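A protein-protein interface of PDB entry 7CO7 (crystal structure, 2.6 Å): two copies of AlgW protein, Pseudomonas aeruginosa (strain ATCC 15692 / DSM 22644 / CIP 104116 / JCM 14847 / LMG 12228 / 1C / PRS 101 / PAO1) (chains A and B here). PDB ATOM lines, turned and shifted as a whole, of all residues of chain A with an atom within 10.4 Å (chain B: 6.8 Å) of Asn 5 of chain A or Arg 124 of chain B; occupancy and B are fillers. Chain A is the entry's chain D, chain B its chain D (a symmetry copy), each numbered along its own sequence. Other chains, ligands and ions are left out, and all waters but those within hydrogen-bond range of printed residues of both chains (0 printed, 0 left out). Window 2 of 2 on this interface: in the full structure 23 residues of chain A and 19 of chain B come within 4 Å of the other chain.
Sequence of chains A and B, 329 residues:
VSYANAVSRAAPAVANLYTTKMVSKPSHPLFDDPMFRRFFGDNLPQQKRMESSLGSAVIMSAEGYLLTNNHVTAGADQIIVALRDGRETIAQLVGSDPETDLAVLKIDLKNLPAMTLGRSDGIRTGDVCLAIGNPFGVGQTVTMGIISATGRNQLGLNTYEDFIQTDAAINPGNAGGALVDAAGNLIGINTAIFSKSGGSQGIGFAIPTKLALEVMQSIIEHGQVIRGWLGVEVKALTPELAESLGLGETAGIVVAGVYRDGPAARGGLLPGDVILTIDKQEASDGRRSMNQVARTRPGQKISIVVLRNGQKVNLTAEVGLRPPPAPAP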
ATOM      1  N   VAL A   1      31.916  12.710 -26.721  1.00  0.00           N
ATOM      2  CA  VAL A   1      30.705  13.517 -26.739  1.00  0.00           C
ATOM      3  C   VAL A   1      30.937  14.715 -25.806  1.00  0.00           C
ATOM      4  O   VAL A   1      32.061  14.951 -25.345  1.00  0.00           O
ATOM      5  CB  VAL A   1      29.456  12.653 -26.352  1.00  0.00           C
ATOM      6  CG1 VAL A   1      29.432  12.341 -24.857  1.00  0.00           C
ATOM      7  CG2 VAL A   1      28.154  13.294 -26.816  1.00  0.00           C
ATOM      8  N   SER A   2      29.892  15.494 -25.549  1.00  0.00           N
ATOM      9  CA  SER A   2      30.046  16.679 -24.721  1.00  0.00           C
ATOM     10  C   SER A   2      28.713  17.041 -24.107  1.00  0.00           C
ATOM     11  O   SER A   2      27.666  16.820 -24.714  1.00  0.00           O
ATOM     12  CB  SER A   2      30.575  17.884 -25.479  1.00  0.00           C
ATOM     13  OG  SER A   2      30.363  19.055 -24.701  1.00  0.00           O
ATOM     14  N   TYR A   3      28.766  17.607 -22.898  1.00  0.00           N
ATOM     15  CA  TYR A   3      27.577  18.052 -22.190  1.00  0.00           C
ATOM     16  C   TYR A   3      27.597  19.550 -21.982  1.00  0.00           C
ATOM     17  O   TYR A   3      26.867  20.064 -21.127  1.00  0.00           O
ATOM     18  CB  TYR A   3      27.435  17.313 -20.856  1.00  0.00           C
ATOM     19  CG  TYR A   3      27.453  15.799 -20.984  1.00  0.00           C
ATOM     20  CD1 TYR A   3      26.283  15.097 -21.245  1.00  0.00           C
ATOM     21  CD2 TYR A   3      28.630  15.075 -20.835  1.00  0.00           C
ATOM     22  CE1 TYR A   3      26.274  13.720 -21.367  1.00  0.00           C
ATOM     23  CE2 TYR A   3      28.631  13.698 -20.955  1.00  0.00           C
ATOM     24  CZ  TYR A   3      27.446  13.025 -21.229  1.00  0.00           C
ATOM     25  OH  TYR A   3      27.436  11.656 -21.349  1.00  0.00           O
ATOM     26  N   ALA A   4      28.409  20.258 -22.777  1.00  0.00           N
ATOM     27  CA  ALA A   4      28.512  21.711 -22.650  1.00  0.00           C
ATOM     28  C   ALA A   4      27.212  22.432 -23.001  1.00  0.00           C
ATOM     29  O   ALA A   4      26.969  23.536 -22.497  1.00  0.00           O
ATOM     30  CB  ALA A   4      29.642  22.239 -23.533  1.00  0.00           C
ATOM     31  N   ASN A   5      26.366  21.851 -23.862  1.00  0.00           N
ATOM     32  CA  ASN A   5      25.086  22.502 -24.148  1.00  0.00           C
ATOM     33  C   ASN A   5      24.120  22.362 -22.979  1.00  0.00           C
ATOM     34  O   ASN A   5      23.435  23.325 -22.618  1.00  0.00           O
ATOM     35  CB  ASN A   5      24.449  21.955 -25.428  1.00  0.00           C
ATOM     36  CG  ASN A   5      25.219  22.334 -26.676  1.00  0.00           C
ATOM     37  OD1 ASN A   5      25.837  23.394 -26.736  1.00  0.00           O
ATOM     38  ND2 ASN A   5      25.163  21.481 -27.689  1.00  0.00           N
ATOM     39  N   ALA A   6      24.044  21.175 -22.372  1.00  0.00           N
ATOM     40  CA  ALA A   6      23.301  21.062 -21.119  1.00  0.00           C
ATOM     41  C   ALA A   6      23.840  22.036 -20.075  1.00  0.00           C
ATOM     42  O   ALA A   6      23.069  22.744 -19.425  1.00  0.00           O
ATOM     43  CB  ALA A   6      23.356  19.631 -20.580  1.00  0.00           C
ATOM     44  N   VAL A   7      25.167  22.116 -19.924  1.00  0.00           N
ATOM     45  CA  VAL A   7      25.735  23.038 -18.940  1.00  0.00           C
ATOM     46  C   VAL A   7      25.312  24.457 -19.254  1.00  0.00           C
ATOM     47  O   VAL A   7      25.043  25.254 -18.349  1.00  0.00           O
ATOM     48  CB  VAL A   7      27.269  22.936 -18.870  1.00  0.00           C
ATOM     49  CG1 VAL A   7      27.808  24.070 -18.006  1.00  0.00           C
ATOM     50  CG2 VAL A   7      27.702  21.587 -18.323  1.00  0.00           C
ATOM     51  N   SER A   8      25.274  24.811 -20.539  1.00  0.00           N
ATOM     52  CA  SER A   8      24.902  26.178 -20.893  1.00  0.00           C
ATOM     53  C   SER A   8      23.440  26.451 -20.579  1.00  0.00           C
ATOM     54  O   SER A   8      23.082  27.571 -20.214  1.00  0.00           O
ATOM     55  CB  SER A   8      25.194  26.442 -22.367  1.00  0.00           C
ATOM     56  OG  SER A   8      26.545  26.169 -22.685  1.00  0.00           O
ATOM     57  N   ARG A   9      22.584  25.440 -20.707  1.00  0.00           N
ATOM     58  CA  ARG A   9      21.151  25.631 -20.482  1.00  0.00           C
ATOM     59  C   ARG A   9      20.808  25.816 -19.014  1.00  0.00           C
ATOM     60  O   ARG A   9      19.947  26.636 -18.678  1.00  0.00           O
ATOM     61  CB  ARG A   9      20.352  24.441 -20.991  1.00  0.00           C
ATOM     62  CG  ARG A   9      20.353  24.256 -22.485  1.00  0.00           C
ATOM     63  CD  ARG A   9      19.313  23.218 -22.786  1.00  0.00           C
ATOM     64  NE  ARG A   9      18.108  23.496 -22.011  1.00  0.00           N
ATOM     65  CZ  ARG A   9      17.304  22.558 -21.526  1.00  0.00           C
ATOM     66  NH1 ARG A   9      16.222  22.905 -20.839  1.00  0.00           N
ATOM     67  NH2 ARG A   9      17.588  21.275 -21.721  1.00  0.00           N
ATOM     68  N   ALA A  10      21.429  25.030 -18.128  1.00  0.00           N
ATOM     69  CA  ALA A  10      21.044  24.974 -16.723  1.00  0.00           C
ATOM     70  C   ALA A  10      21.972  25.768 -15.813  1.00  0.00           C
ATOM     71  O   ALA A  10      21.493  26.417 -14.862  1.00  0.00           O
ATOM     72  CB  ALA A  10      20.992  23.507 -16.258  1.00  0.00           C
ATOM     73  N   ALA A  11      23.268  25.771 -16.115  1.00  0.00           N
ATOM     74  CA  ALA A  11      24.224  26.430 -15.237  1.00  0.00           C
ATOM     75  C   ALA A  11      23.787  27.840 -14.860  1.00  0.00           C
ATOM     76  O   ALA A  11      23.868  28.177 -13.669  1.00  0.00           O
ATOM     77  CB  ALA A  11      25.605  26.431 -15.891  1.00  0.00           C
ATOM     78  N   PRO A  12      23.282  28.684 -15.760  1.00  0.00           N
ATOM     79  CA  PRO A  12      22.942  30.042 -15.317  1.00  0.00           C
ATOM     80  C   PRO A  12      21.853  30.069 -14.268  1.00  0.00           C
ATOM     81  O   PRO A  12      21.737  31.069 -13.562  1.00  0.00           O
ATOM     82  CB  PRO A  12      22.508  30.734 -16.615  1.00  0.00           C
ATOM     83  CG  PRO A  12      23.064  29.912 -17.688  1.00  0.00           C
ATOM     84  CD  PRO A  12      23.011  28.517 -17.199  1.00  0.00           C
ATOM     85  N   ARG A  84      25.389  33.252 -11.372  1.00  0.00           N
ATOM     86  CA  ARG A  84      26.459  32.874 -12.286  1.00  0.00           C
ATOM     87  C   ARG A  84      27.033  34.100 -12.991  1.00  0.00           C
ATOM     88  O   ARG A  84      28.249  34.180 -13.200  1.00  0.00           O
ATOM     89  CB  ARG A  84      25.954  31.846 -13.303  1.00  0.00           C
ATOM     90  CG  ARG A  84      27.044  31.080 -14.064  1.00  0.00           C
ATOM     91  CD  ARG A  84      26.489  30.445 -15.339  1.00  0.00           C
ATOM     92  NE  ARG A  84      27.508  29.694 -16.065  1.00  0.00           N
ATOM     93  CZ  ARG A  84      27.586  29.607 -17.390  1.00  0.00           C
ATOM     94  NH1 ARG A  84      28.556  28.890 -17.945  1.00  0.00           N
ATOM     95  NH2 ARG A  84      26.710  30.245 -18.160  1.00  0.00           N
ATOM     96  N   MET A 115      15.487  27.388 -14.280  1.00  0.00           N
ATOM     97  CA  MET A 115      15.769  25.994 -14.564  1.00  0.00           C
ATOM     98  C   MET A 115      14.584  25.364 -15.265  1.00  0.00           C
ATOM     99  O   MET A 115      13.457  25.449 -14.786  1.00  0.00           O
ATOM    100  CB  MET A 115      16.068  25.255 -13.260  1.00  0.00           C
ATOM    101  CG  MET A 115      16.600  23.853 -13.425  1.00  0.00           C
ATOM    102  SD  MET A 115      18.241  23.881 -14.136  1.00  0.00           S
ATOM    103  CE  MET A 115      19.055  25.042 -13.056  1.00  0.00           C
ATOM    104  N   THR A 116      14.838  24.763 -16.410  1.00  0.00           N
ATOM    105  CA  THR A 116      13.882  23.864 -17.023  1.00  0.00           C
ATOM    106  C   THR A 116      13.771  22.606 -16.184  1.00  0.00           C
ATOM    107  O   THR A 116      14.783  21.966 -15.899  1.00  0.00           O
ATOM    108  CB  THR A 116      14.363  23.507 -18.422  1.00  0.00           C
ATOM    109  OG1 THR A 116      14.705  24.717 -19.098  1.00  0.00           O
ATOM    110  CG2 THR A 116      13.297  22.740 -19.204  1.00  0.00           C
ATOM    111  N   LEU A 130      24.371  15.329 -14.318  1.00  0.00           N
ATOM    112  CA  LEU A 130      25.359  16.335 -14.018  1.00  0.00           C
ATOM    113  C   LEU A 130      24.967  17.008 -12.715  1.00  0.00           C
ATOM    114  O   LEU A 130      23.787  17.207 -12.430  1.00  0.00           O
ATOM    115  CB  LEU A 130      25.462  17.360 -15.149  1.00  0.00           C
ATOM    116  CG  LEU A 130      25.783  16.904 -16.573  1.00  0.00           C
ATOM    117  CD1 LEU A 130      25.661  18.082 -17.511  1.00  0.00           C
ATOM    118  CD2 LEU A 130      27.158  16.289 -16.726  1.00  0.00           C
ATOM    119  N   ILE A 132      25.629  20.391 -10.275  1.00  0.00           N
ATOM    120  CA  ILE A 132      26.073  21.778 -10.320  1.00  0.00           C
ATOM    121  C   ILE A 132      25.940  22.404  -8.933  1.00  0.00           C
ATOM    122  O   ILE A 132      24.832  22.502  -8.388  1.00  0.00           O
ATOM    123  CB  ILE A 132      25.253  22.616 -11.314  1.00  0.00           C
ATOM    124  CG1 ILE A 132      25.194  21.988 -12.702  1.00  0.00           C
ATOM    125  CG2 ILE A 132      25.792  24.042 -11.361  1.00  0.00           C
ATOM    126  CD1 ILE A 132      24.720  22.988 -13.740  1.00  0.00           C
ATOM    127  N   VAL A 142      30.798  21.982 -12.459  1.00  0.00           N
ATOM    128  CA  VAL A 142      29.911  20.952 -12.983  1.00  0.00           C
ATOM    129  C   VAL A 142      30.636  19.618 -12.896  1.00  0.00           C
ATOM    130  O   VAL A 142      31.795  19.515 -13.294  1.00  0.00           O
ATOM    131  CB  VAL A 142      29.510  21.240 -14.440  1.00  0.00           C
ATOM    132  CG1 VAL A 142      28.627  20.125 -14.983  1.00  0.00           C
ATOM    133  CG2 VAL A 142      28.843  22.569 -14.557  1.00  0.00           C
ATOM    134  N   VAL A 180      21.003  17.396 -12.692  1.00  0.00           N
ATOM    135  CA  VAL A 180      20.447  17.697 -14.000  1.00  0.00           C
ATOM    136  C   VAL A 180      20.691  16.509 -14.916  1.00  0.00           C
ATOM    137  O   VAL A 180      21.687  15.796 -14.770  1.00  0.00           O
ATOM    138  CB  VAL A 180      21.092  18.981 -14.561  1.00  0.00           C
ATOM    139  CG1 VAL A 180      21.604  18.772 -15.961  1.00  0.00           C
ATOM    140  CG2 VAL A 180      20.122  20.113 -14.489  1.00  0.00           C
ATOM    141  N   ASP A 181      19.776  16.289 -15.860  1.00  0.00           N
ATOM    142  CA  ASP A 181      19.923  15.190 -16.803  1.00  0.00           C
ATOM    143  C   ASP A 181      20.696  15.634 -18.045  1.00  0.00           C
ATOM    144  O   ASP A 181      21.091  16.798 -18.192  1.00  0.00           O
ATOM    145  CB  ASP A 181      18.556  14.616 -17.165  1.00  0.00           C
ATOM    146  CG  ASP A 181      17.713  15.549 -18.039  1.00  0.00           C
ATOM    147  OD1 ASP A 181      18.172  16.669 -18.409  1.00  0.00           O
ATOM    148  OD2 ASP A 181      16.569  15.154 -18.356  1.00  0.00           O
ATOM    149  N   ALA A 182      20.913  14.686 -18.959  1.00  0.00           N
ATOM    150  CA  ALA A 182      21.831  14.940 -20.068  1.00  0.00           C
ATOM    151  C   ALA A 182      21.352  16.082 -20.945  1.00  0.00           C
ATOM    152  O   ALA A 182      22.168  16.796 -21.538  1.00  0.00           O
ATOM    153  CB  ALA A 182      22.007  13.679 -20.902  1.00  0.00           C
ATOM    154  N   ALA A 183      20.026  16.250 -21.051  1.00  0.00           N
ATOM    155  CA  ALA A 183      19.421  17.382 -21.752  1.00  0.00           C
ATOM    156  C   ALA A 183      19.668  18.705 -21.047  1.00  0.00           C
ATOM    157  O   ALA A 183      19.633  19.754 -21.693  1.00  0.00           O
ATOM    158  CB  ALA A 183      17.908  17.172 -21.893  1.00  0.00           C
ATOM    159  N   GLY A 184      19.882  18.691 -19.738  1.00  0.00           N
ATOM    160  CA  GLY A 184      20.007  19.916 -18.989  1.00  0.00           C
ATOM    161  C   GLY A 184      18.818  20.290 -18.124  1.00  0.00           C
ATOM    162  O   GLY A 184      18.760  21.432 -17.660  1.00  0.00           O
ATOM    163  N   ASN A 185      17.887  19.367 -17.860  1.00  0.00           N
ATOM    164  CA  ASN A 185      16.699  19.648 -17.050  1.00  0.00           C
ATOM    165  C   ASN A 185      16.861  19.174 -15.613  1.00  0.00           C
ATOM    166  O   ASN A 185      17.418  18.101 -15.363  1.00  0.00           O
ATOM    167  CB  ASN A 185      15.447  18.986 -17.648  1.00  0.00           C
ATOM    168  CG  ASN A 185      15.424  19.063 -19.152  1.00  0.00           C
ATOM    169  OD1 ASN A 185      15.712  20.102 -19.734  1.00  0.00           O
ATOM    170  ND2 ASN A 185      15.116  17.932 -19.799  1.00  0.00           N
ATOM    171  N   SER B 120      43.489  25.011 -25.684  1.00  0.00           N
ATOM    172  CA  SER B 120      42.935  25.291 -24.367  1.00  0.00           C
ATOM    173  C   SER B 120      41.753  26.243 -24.436  1.00  0.00           C
ATOM    174  O   SER B 120      40.747  26.026 -23.757  1.00  0.00           O
ATOM    175  CB  SER B 120      44.016  25.885 -23.469  1.00  0.00           C
ATOM    176  OG  SER B 120      45.303  25.372 -23.804  1.00  0.00           O
ATOM    177  N   ASP B 121      41.855  27.319 -25.227  1.00  0.00           N
ATOM    178  CA  ASP B 121      40.758  28.287 -25.282  1.00  0.00           C
ATOM    179  C   ASP B 121      39.491  27.720 -25.879  1.00  0.00           C
ATOM    180  O   ASP B 121      38.443  28.366 -25.782  1.00  0.00           O
ATOM    181  CB  ASP B 121      41.123  29.503 -26.100  1.00  0.00           C
ATOM    182  CG  ASP B 121      41.999  30.417 -25.367  1.00  0.00           C
ATOM    183  OD1 ASP B 121      41.999  30.397 -24.133  1.00  0.00           O
ATOM    184  OD2 ASP B 121      42.723  31.175 -26.026  1.00  0.00           O
ATOM    185  N   GLY B 122      39.562  26.570 -26.529  1.00  0.00           N
ATOM    186  CA  GLY B 122      38.382  26.057 -27.172  1.00  0.00           C
ATOM    187  C   GLY B 122      37.572  25.106 -26.342  1.00  0.00           C
ATOM    188  O   GLY B 122      36.474  24.730 -26.759  1.00  0.00           O
ATOM    189  N   ILE B 123      38.077  24.700 -25.173  1.00  0.00           N
ATOM    190  CA  ILE B 123      37.329  23.780 -24.331  1.00  0.00           C
ATOM    191  C   ILE B 123      36.147  24.508 -23.724  1.00  0.00           C
ATOM    192  O   ILE B 123      36.219  25.698 -23.395  1.00  0.00           O
ATOM    193  CB  ILE B 123      38.201  23.177 -23.217  1.00  0.00           C
ATOM    194  CG1 ILE B 123      38.469  24.227 -22.134  1.00  0.00           C
ATOM    195  CG2 ILE B 123      39.494  22.624 -23.763  1.00  0.00           C
ATOM    196  CD1 ILE B 123      39.474  23.740 -21.087  1.00  0.00           C
ATOM    197  N   ARG B 124      35.049  23.782 -23.555  1.00  0.00           N
ATOM    198  CA  ARG B 124      33.892  24.292 -22.832  1.00  0.00           C
ATOM    199  C   ARG B 124      33.528  23.388 -21.660  1.00  0.00           C
ATOM    200  O   ARG B 124      33.545  22.155 -21.771  1.00  0.00           O
ATOM    201  CB  ARG B 124      32.677  24.427 -23.756  1.00  0.00           C
ATOM    202  CG  ARG B 124      32.997  24.449 -25.228  1.00  0.00           C
ATOM    203  CD  ARG B 124      31.706  24.381 -26.014  1.00  0.00           C
ATOM    204  NE  ARG B 124      30.710  25.281 -25.437  1.00  0.00           N
ATOM    205  CZ  ARG B 124      29.396  25.101 -25.532  1.00  0.00           C
ATOM    206  NH1 ARG B 124      28.913  24.046 -26.184  1.00  0.00           N
ATOM    207  NH2 ARG B 124      28.564  25.974 -24.967  1.00  0.00           N
ATOM    208  N   THR B 125      33.186  24.018 -20.536  1.00  0.00           N
ATOM    209  CA  THR B 125      32.656  23.271 -19.404  1.00  0.00           C
ATOM    210  C   THR B 125      31.586  22.290 -19.863  1.00  0.00           C
ATOM    211  O   THR B 125      30.563  22.688 -20.408  1.00  0.00           O
ATOM    212  CB  THR B 125      32.064  24.226 -18.373  1.00  0.00           C
ATOM    213  OG1 THR B 125      33.084  25.093 -17.881  1.00  0.00           O
ATOM    214  CG2 THR B 125      31.476  23.471 -17.215  1.00  0.00           C
ATOM    215  N   GLY B 126      31.788  21.023 -19.584  1.00  0.00           N
ATOM    216  CA  GLY B 126      30.900  19.994 -20.048  1.00  0.00           C
ATOM    217  C   GLY B 126      31.589  19.015 -20.947  1.00  0.00           C
ATOM    218  O   GLY B 126      31.124  17.882 -21.054  1.00  0.00           O
ATOM    219  N   ASP B 127      32.687  19.409 -21.594  1.00  0.00           N
ATOM    220  CA  ASP B 127      33.376  18.497 -22.500  1.00  0.00           C
ATOM    221  C   ASP B 127      33.972  17.349 -21.718  1.00  0.00           C
ATOM    222  O   ASP B 127      34.522  17.533 -20.645  1.00  0.00           O
ATOM    223  CB  ASP B 127      34.507  19.191 -23.268  1.00  0.00           C
ATOM    224  CG  ASP B 127      34.030  20.360 -24.103  1.00  0.00           C
ATOM    225  OD1 ASP B 127      32.809  20.423 -24.393  1.00  0.00           O
ATOM    226  OD2 ASP B 127      34.899  21.199 -24.470  1.00  0.00           O
ATOM    227  N   VAL B 128      33.887  16.157 -22.268  1.00  0.00           N
ATOM    228  CA  VAL B 128      34.563  15.033 -21.656  1.00  0.00           C
ATOM    229  C   VAL B 128      36.074  15.199 -21.777  1.00  0.00           C
ATOM    230  O   VAL B 128      36.597  15.762 -22.739  1.00  0.00           O
ATOM    231  CB  VAL B 128      34.085  13.730 -22.306  1.00  0.00           C
ATOM    232  CG1 VAL B 128      34.984  12.567 -21.920  1.00  0.00           C
ATOM    233  CG2 VAL B 128      32.686  13.456 -21.903  1.00  0.00           C
ATOM    234  N   ILE B 146      34.647  15.247 -16.837  1.00  0.00           N
ATOM    235  CA  ILE B 146      34.325  16.379 -17.702  1.00  0.00           C
ATOM    236  C   ILE B 146      35.010  17.634 -17.195  1.00  0.00           C
ATOM    237  O   ILE B 146      35.267  17.790 -16.005  1.00  0.00           O
ATOM    238  CB  ILE B 146      32.821  16.683 -17.797  1.00  0.00           C
ATOM    239  CG1 ILE B 146      32.364  17.405 -16.521  1.00  0.00           C
ATOM    240  CG2 ILE B 146      32.020  15.451 -18.083  1.00  0.00           C
ATOM    241  CD1 ILE B 146      30.882  17.583 -16.448  1.00  0.00           C
ATOM    242  N   ILE B 147      35.256  18.565 -18.109  1.00  0.00           N
ATOM    243  CA  ILE B 147      35.675  19.887 -17.695  1.00  0.00           C
ATOM    244  C   ILE B 147      34.611  20.456 -16.773  1.00  0.00           C
ATOM    245  O   ILE B 147      33.501  20.761 -17.216  1.00  0.00           O
ATOM    246  CB  ILE B 147      35.880  20.797 -18.914  1.00  0.00           C
ATOM    247  CG1 ILE B 147      36.632  20.087 -20.038  1.00  0.00           C
ATOM    248  CG2 ILE B 147      36.665  22.014 -18.524  1.00  0.00           C
ATOM    249  CD1 ILE B 147      38.112  20.154 -19.898  1.00  0.00           C
ATOM    250  N   SER B 148      34.960  20.654 -15.500  1.00  0.00           N
ATOM    251  CA  SER B 148      34.066  21.206 -14.496  1.00  0.00           C
ATOM    252  C   SER B 148      33.987  22.730 -14.522  1.00  0.00           C
ATOM    253  O   SER B 148      32.893  23.278 -14.333  1.00  0.00           O
ATOM    254  CB  SER B 148      34.512  20.717 -13.117  1.00  0.00           C
ATOM    255  OG  SER B 148      34.646  19.304 -13.098  1.00  0.00           O
ATOM    256  N   THR B 150      36.488  26.556 -16.011  1.00  0.00           N
ATOM    257  CA  THR B 150      37.694  26.992 -16.699  1.00  0.00           C
ATOM    258  C   THR B 150      38.202  28.288 -16.091  1.00  0.00           C
ATOM    259  O   THR B 150      37.504  28.965 -15.336  1.00  0.00           O
ATOM    260  CB  THR B 150      37.483  27.146 -18.229  1.00  0.00           C
ATOM    261  OG1 THR B 150      36.294  27.883 -18.501  1.00  0.00           O
ATOM    262  CG2 THR B 150      37.375  25.773 -18.900  1.00  0.00           C
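NH2 of Arg 124 of chain B is in hydrogen-bond range of OG of Ser 8 of chain A (3.1 Å).
The backbone NH (N) of Tyr 3 of chain A sits at hydrogen-bond distance from the backbone carbonyl oxygen (O) of Gly 126 of chain B, 3.0 Å away.
OD1 of Asp 127 of chain B sits at hydrogen-bond distance from OG of Ser 2 of chain A.
OD1 of Asn 5 of chain A lies within hydrogen-bond range of NH1 of Arg 124 of chain B (3.2 Å).
The backbone carbonyl oxygen of Val 142 of chain A lies within hydrogen-bond range of the side-chain hydroxyl of Ser 148 of chain B (2.9 Å).
The backbone NH (N) of Gly 126 of chain B lies within hydrogen-bond range of the backbone carbonyl oxygen (O) of Ile 147 of chain B (2.9 Å).
The backbone carbonyl oxygen of Ile 146 of chain B lies within hydrogen-bond range of the side-chain hydroxyl of Ser 148 of chain B (3.3 Å).
The side-chain hydroxyl of Ser 8 of chain A sits at hydrogen-bond distance from the backbone carbonyl oxygen of Ala 4 of chain A (2.7 Å).
The backbone NH (N) of Arg 124 of chain B sits at hydrogen-bond distance from the side-chain carboxylate (OD2) of Asp 127 of chain B, 2.7 Å away.
O of Asp 127 of chain B is in hydrogen-bond range of N of Ile 147 of chain B, 2.8 Å away.
The backbone NH (N) of Leu 130 of chain A lies within hydrogen-bond range of the backbone carbonyl oxygen (O) of Val 180 of chain A (2.8 Å).
Among the printed residues, pairs that only touch across the chains: Val 1 of chain A with Val 128 of chain B, Ser 2 of chain A with Gly 126 of chain B, Ala 4 of chain A with Arg 124 of chain B, Ala 4 of chain A with Thr 125 of chain B, Ala 4 of chain A with Gly 126 of chain B, Ala 4 of chain A with Asp 127 of chain B, Val 7 of chain A with Thr 125 of chain B, Val 7 of chain A with Gly 126 of chain B, Leu 130 of chain A with Ile 146 of chain B, Val 142 of chain A with Thr 125 of chain B and Val 142 of chain A with Ile 146 of chain B.
Printed residues of chain B within 4 Å of Asn 5 of chain A: Arg 124.
No residue of chain A comes within 4 Å of Ile 123 of chain B.
Thr 125 of chain B touches just these residues of chain A: Ala 4, Val 7 and Val 142.
Asp 127 of chain B touches just these residues of chain A: Ser 2 (2.8 Å) and Ala 4 (3.8 Å).
Of the printed residues of chain B, Leu 130 of chain A touches Ile 146.
Of the printed residues of chain B, Tyr 3 of chain A touches Gly 126.
Ala 182 of chain A touches none of the printed residues of chain B.
Asp 181 of chain A touches none of the printed residues of chain B.
The nearest residue of chain B that does not touch Asn 5 of chain A is Thr 125 of chain B (5.5 Å).
Of the 13 printed residues of chain B, 7 touch a printed residue of chain A.
Hydrophobic or aromatic side chains of chain A within 4 Å of the printed part of chain B: Tyr 3, Ala 4, Val 7, Leu 130 and Val 142.
Along chain A the printed residues that touch a printed residue of chain B span positions 1 to 142.
Among the printed residues, 16 pairs touch across the chains.
Among the printed residues, no Asp or Glu carboxylate lies within 4 Å of a Lys or Arg side-chain nitrogen of the other chain.
No position is printed for both chains.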
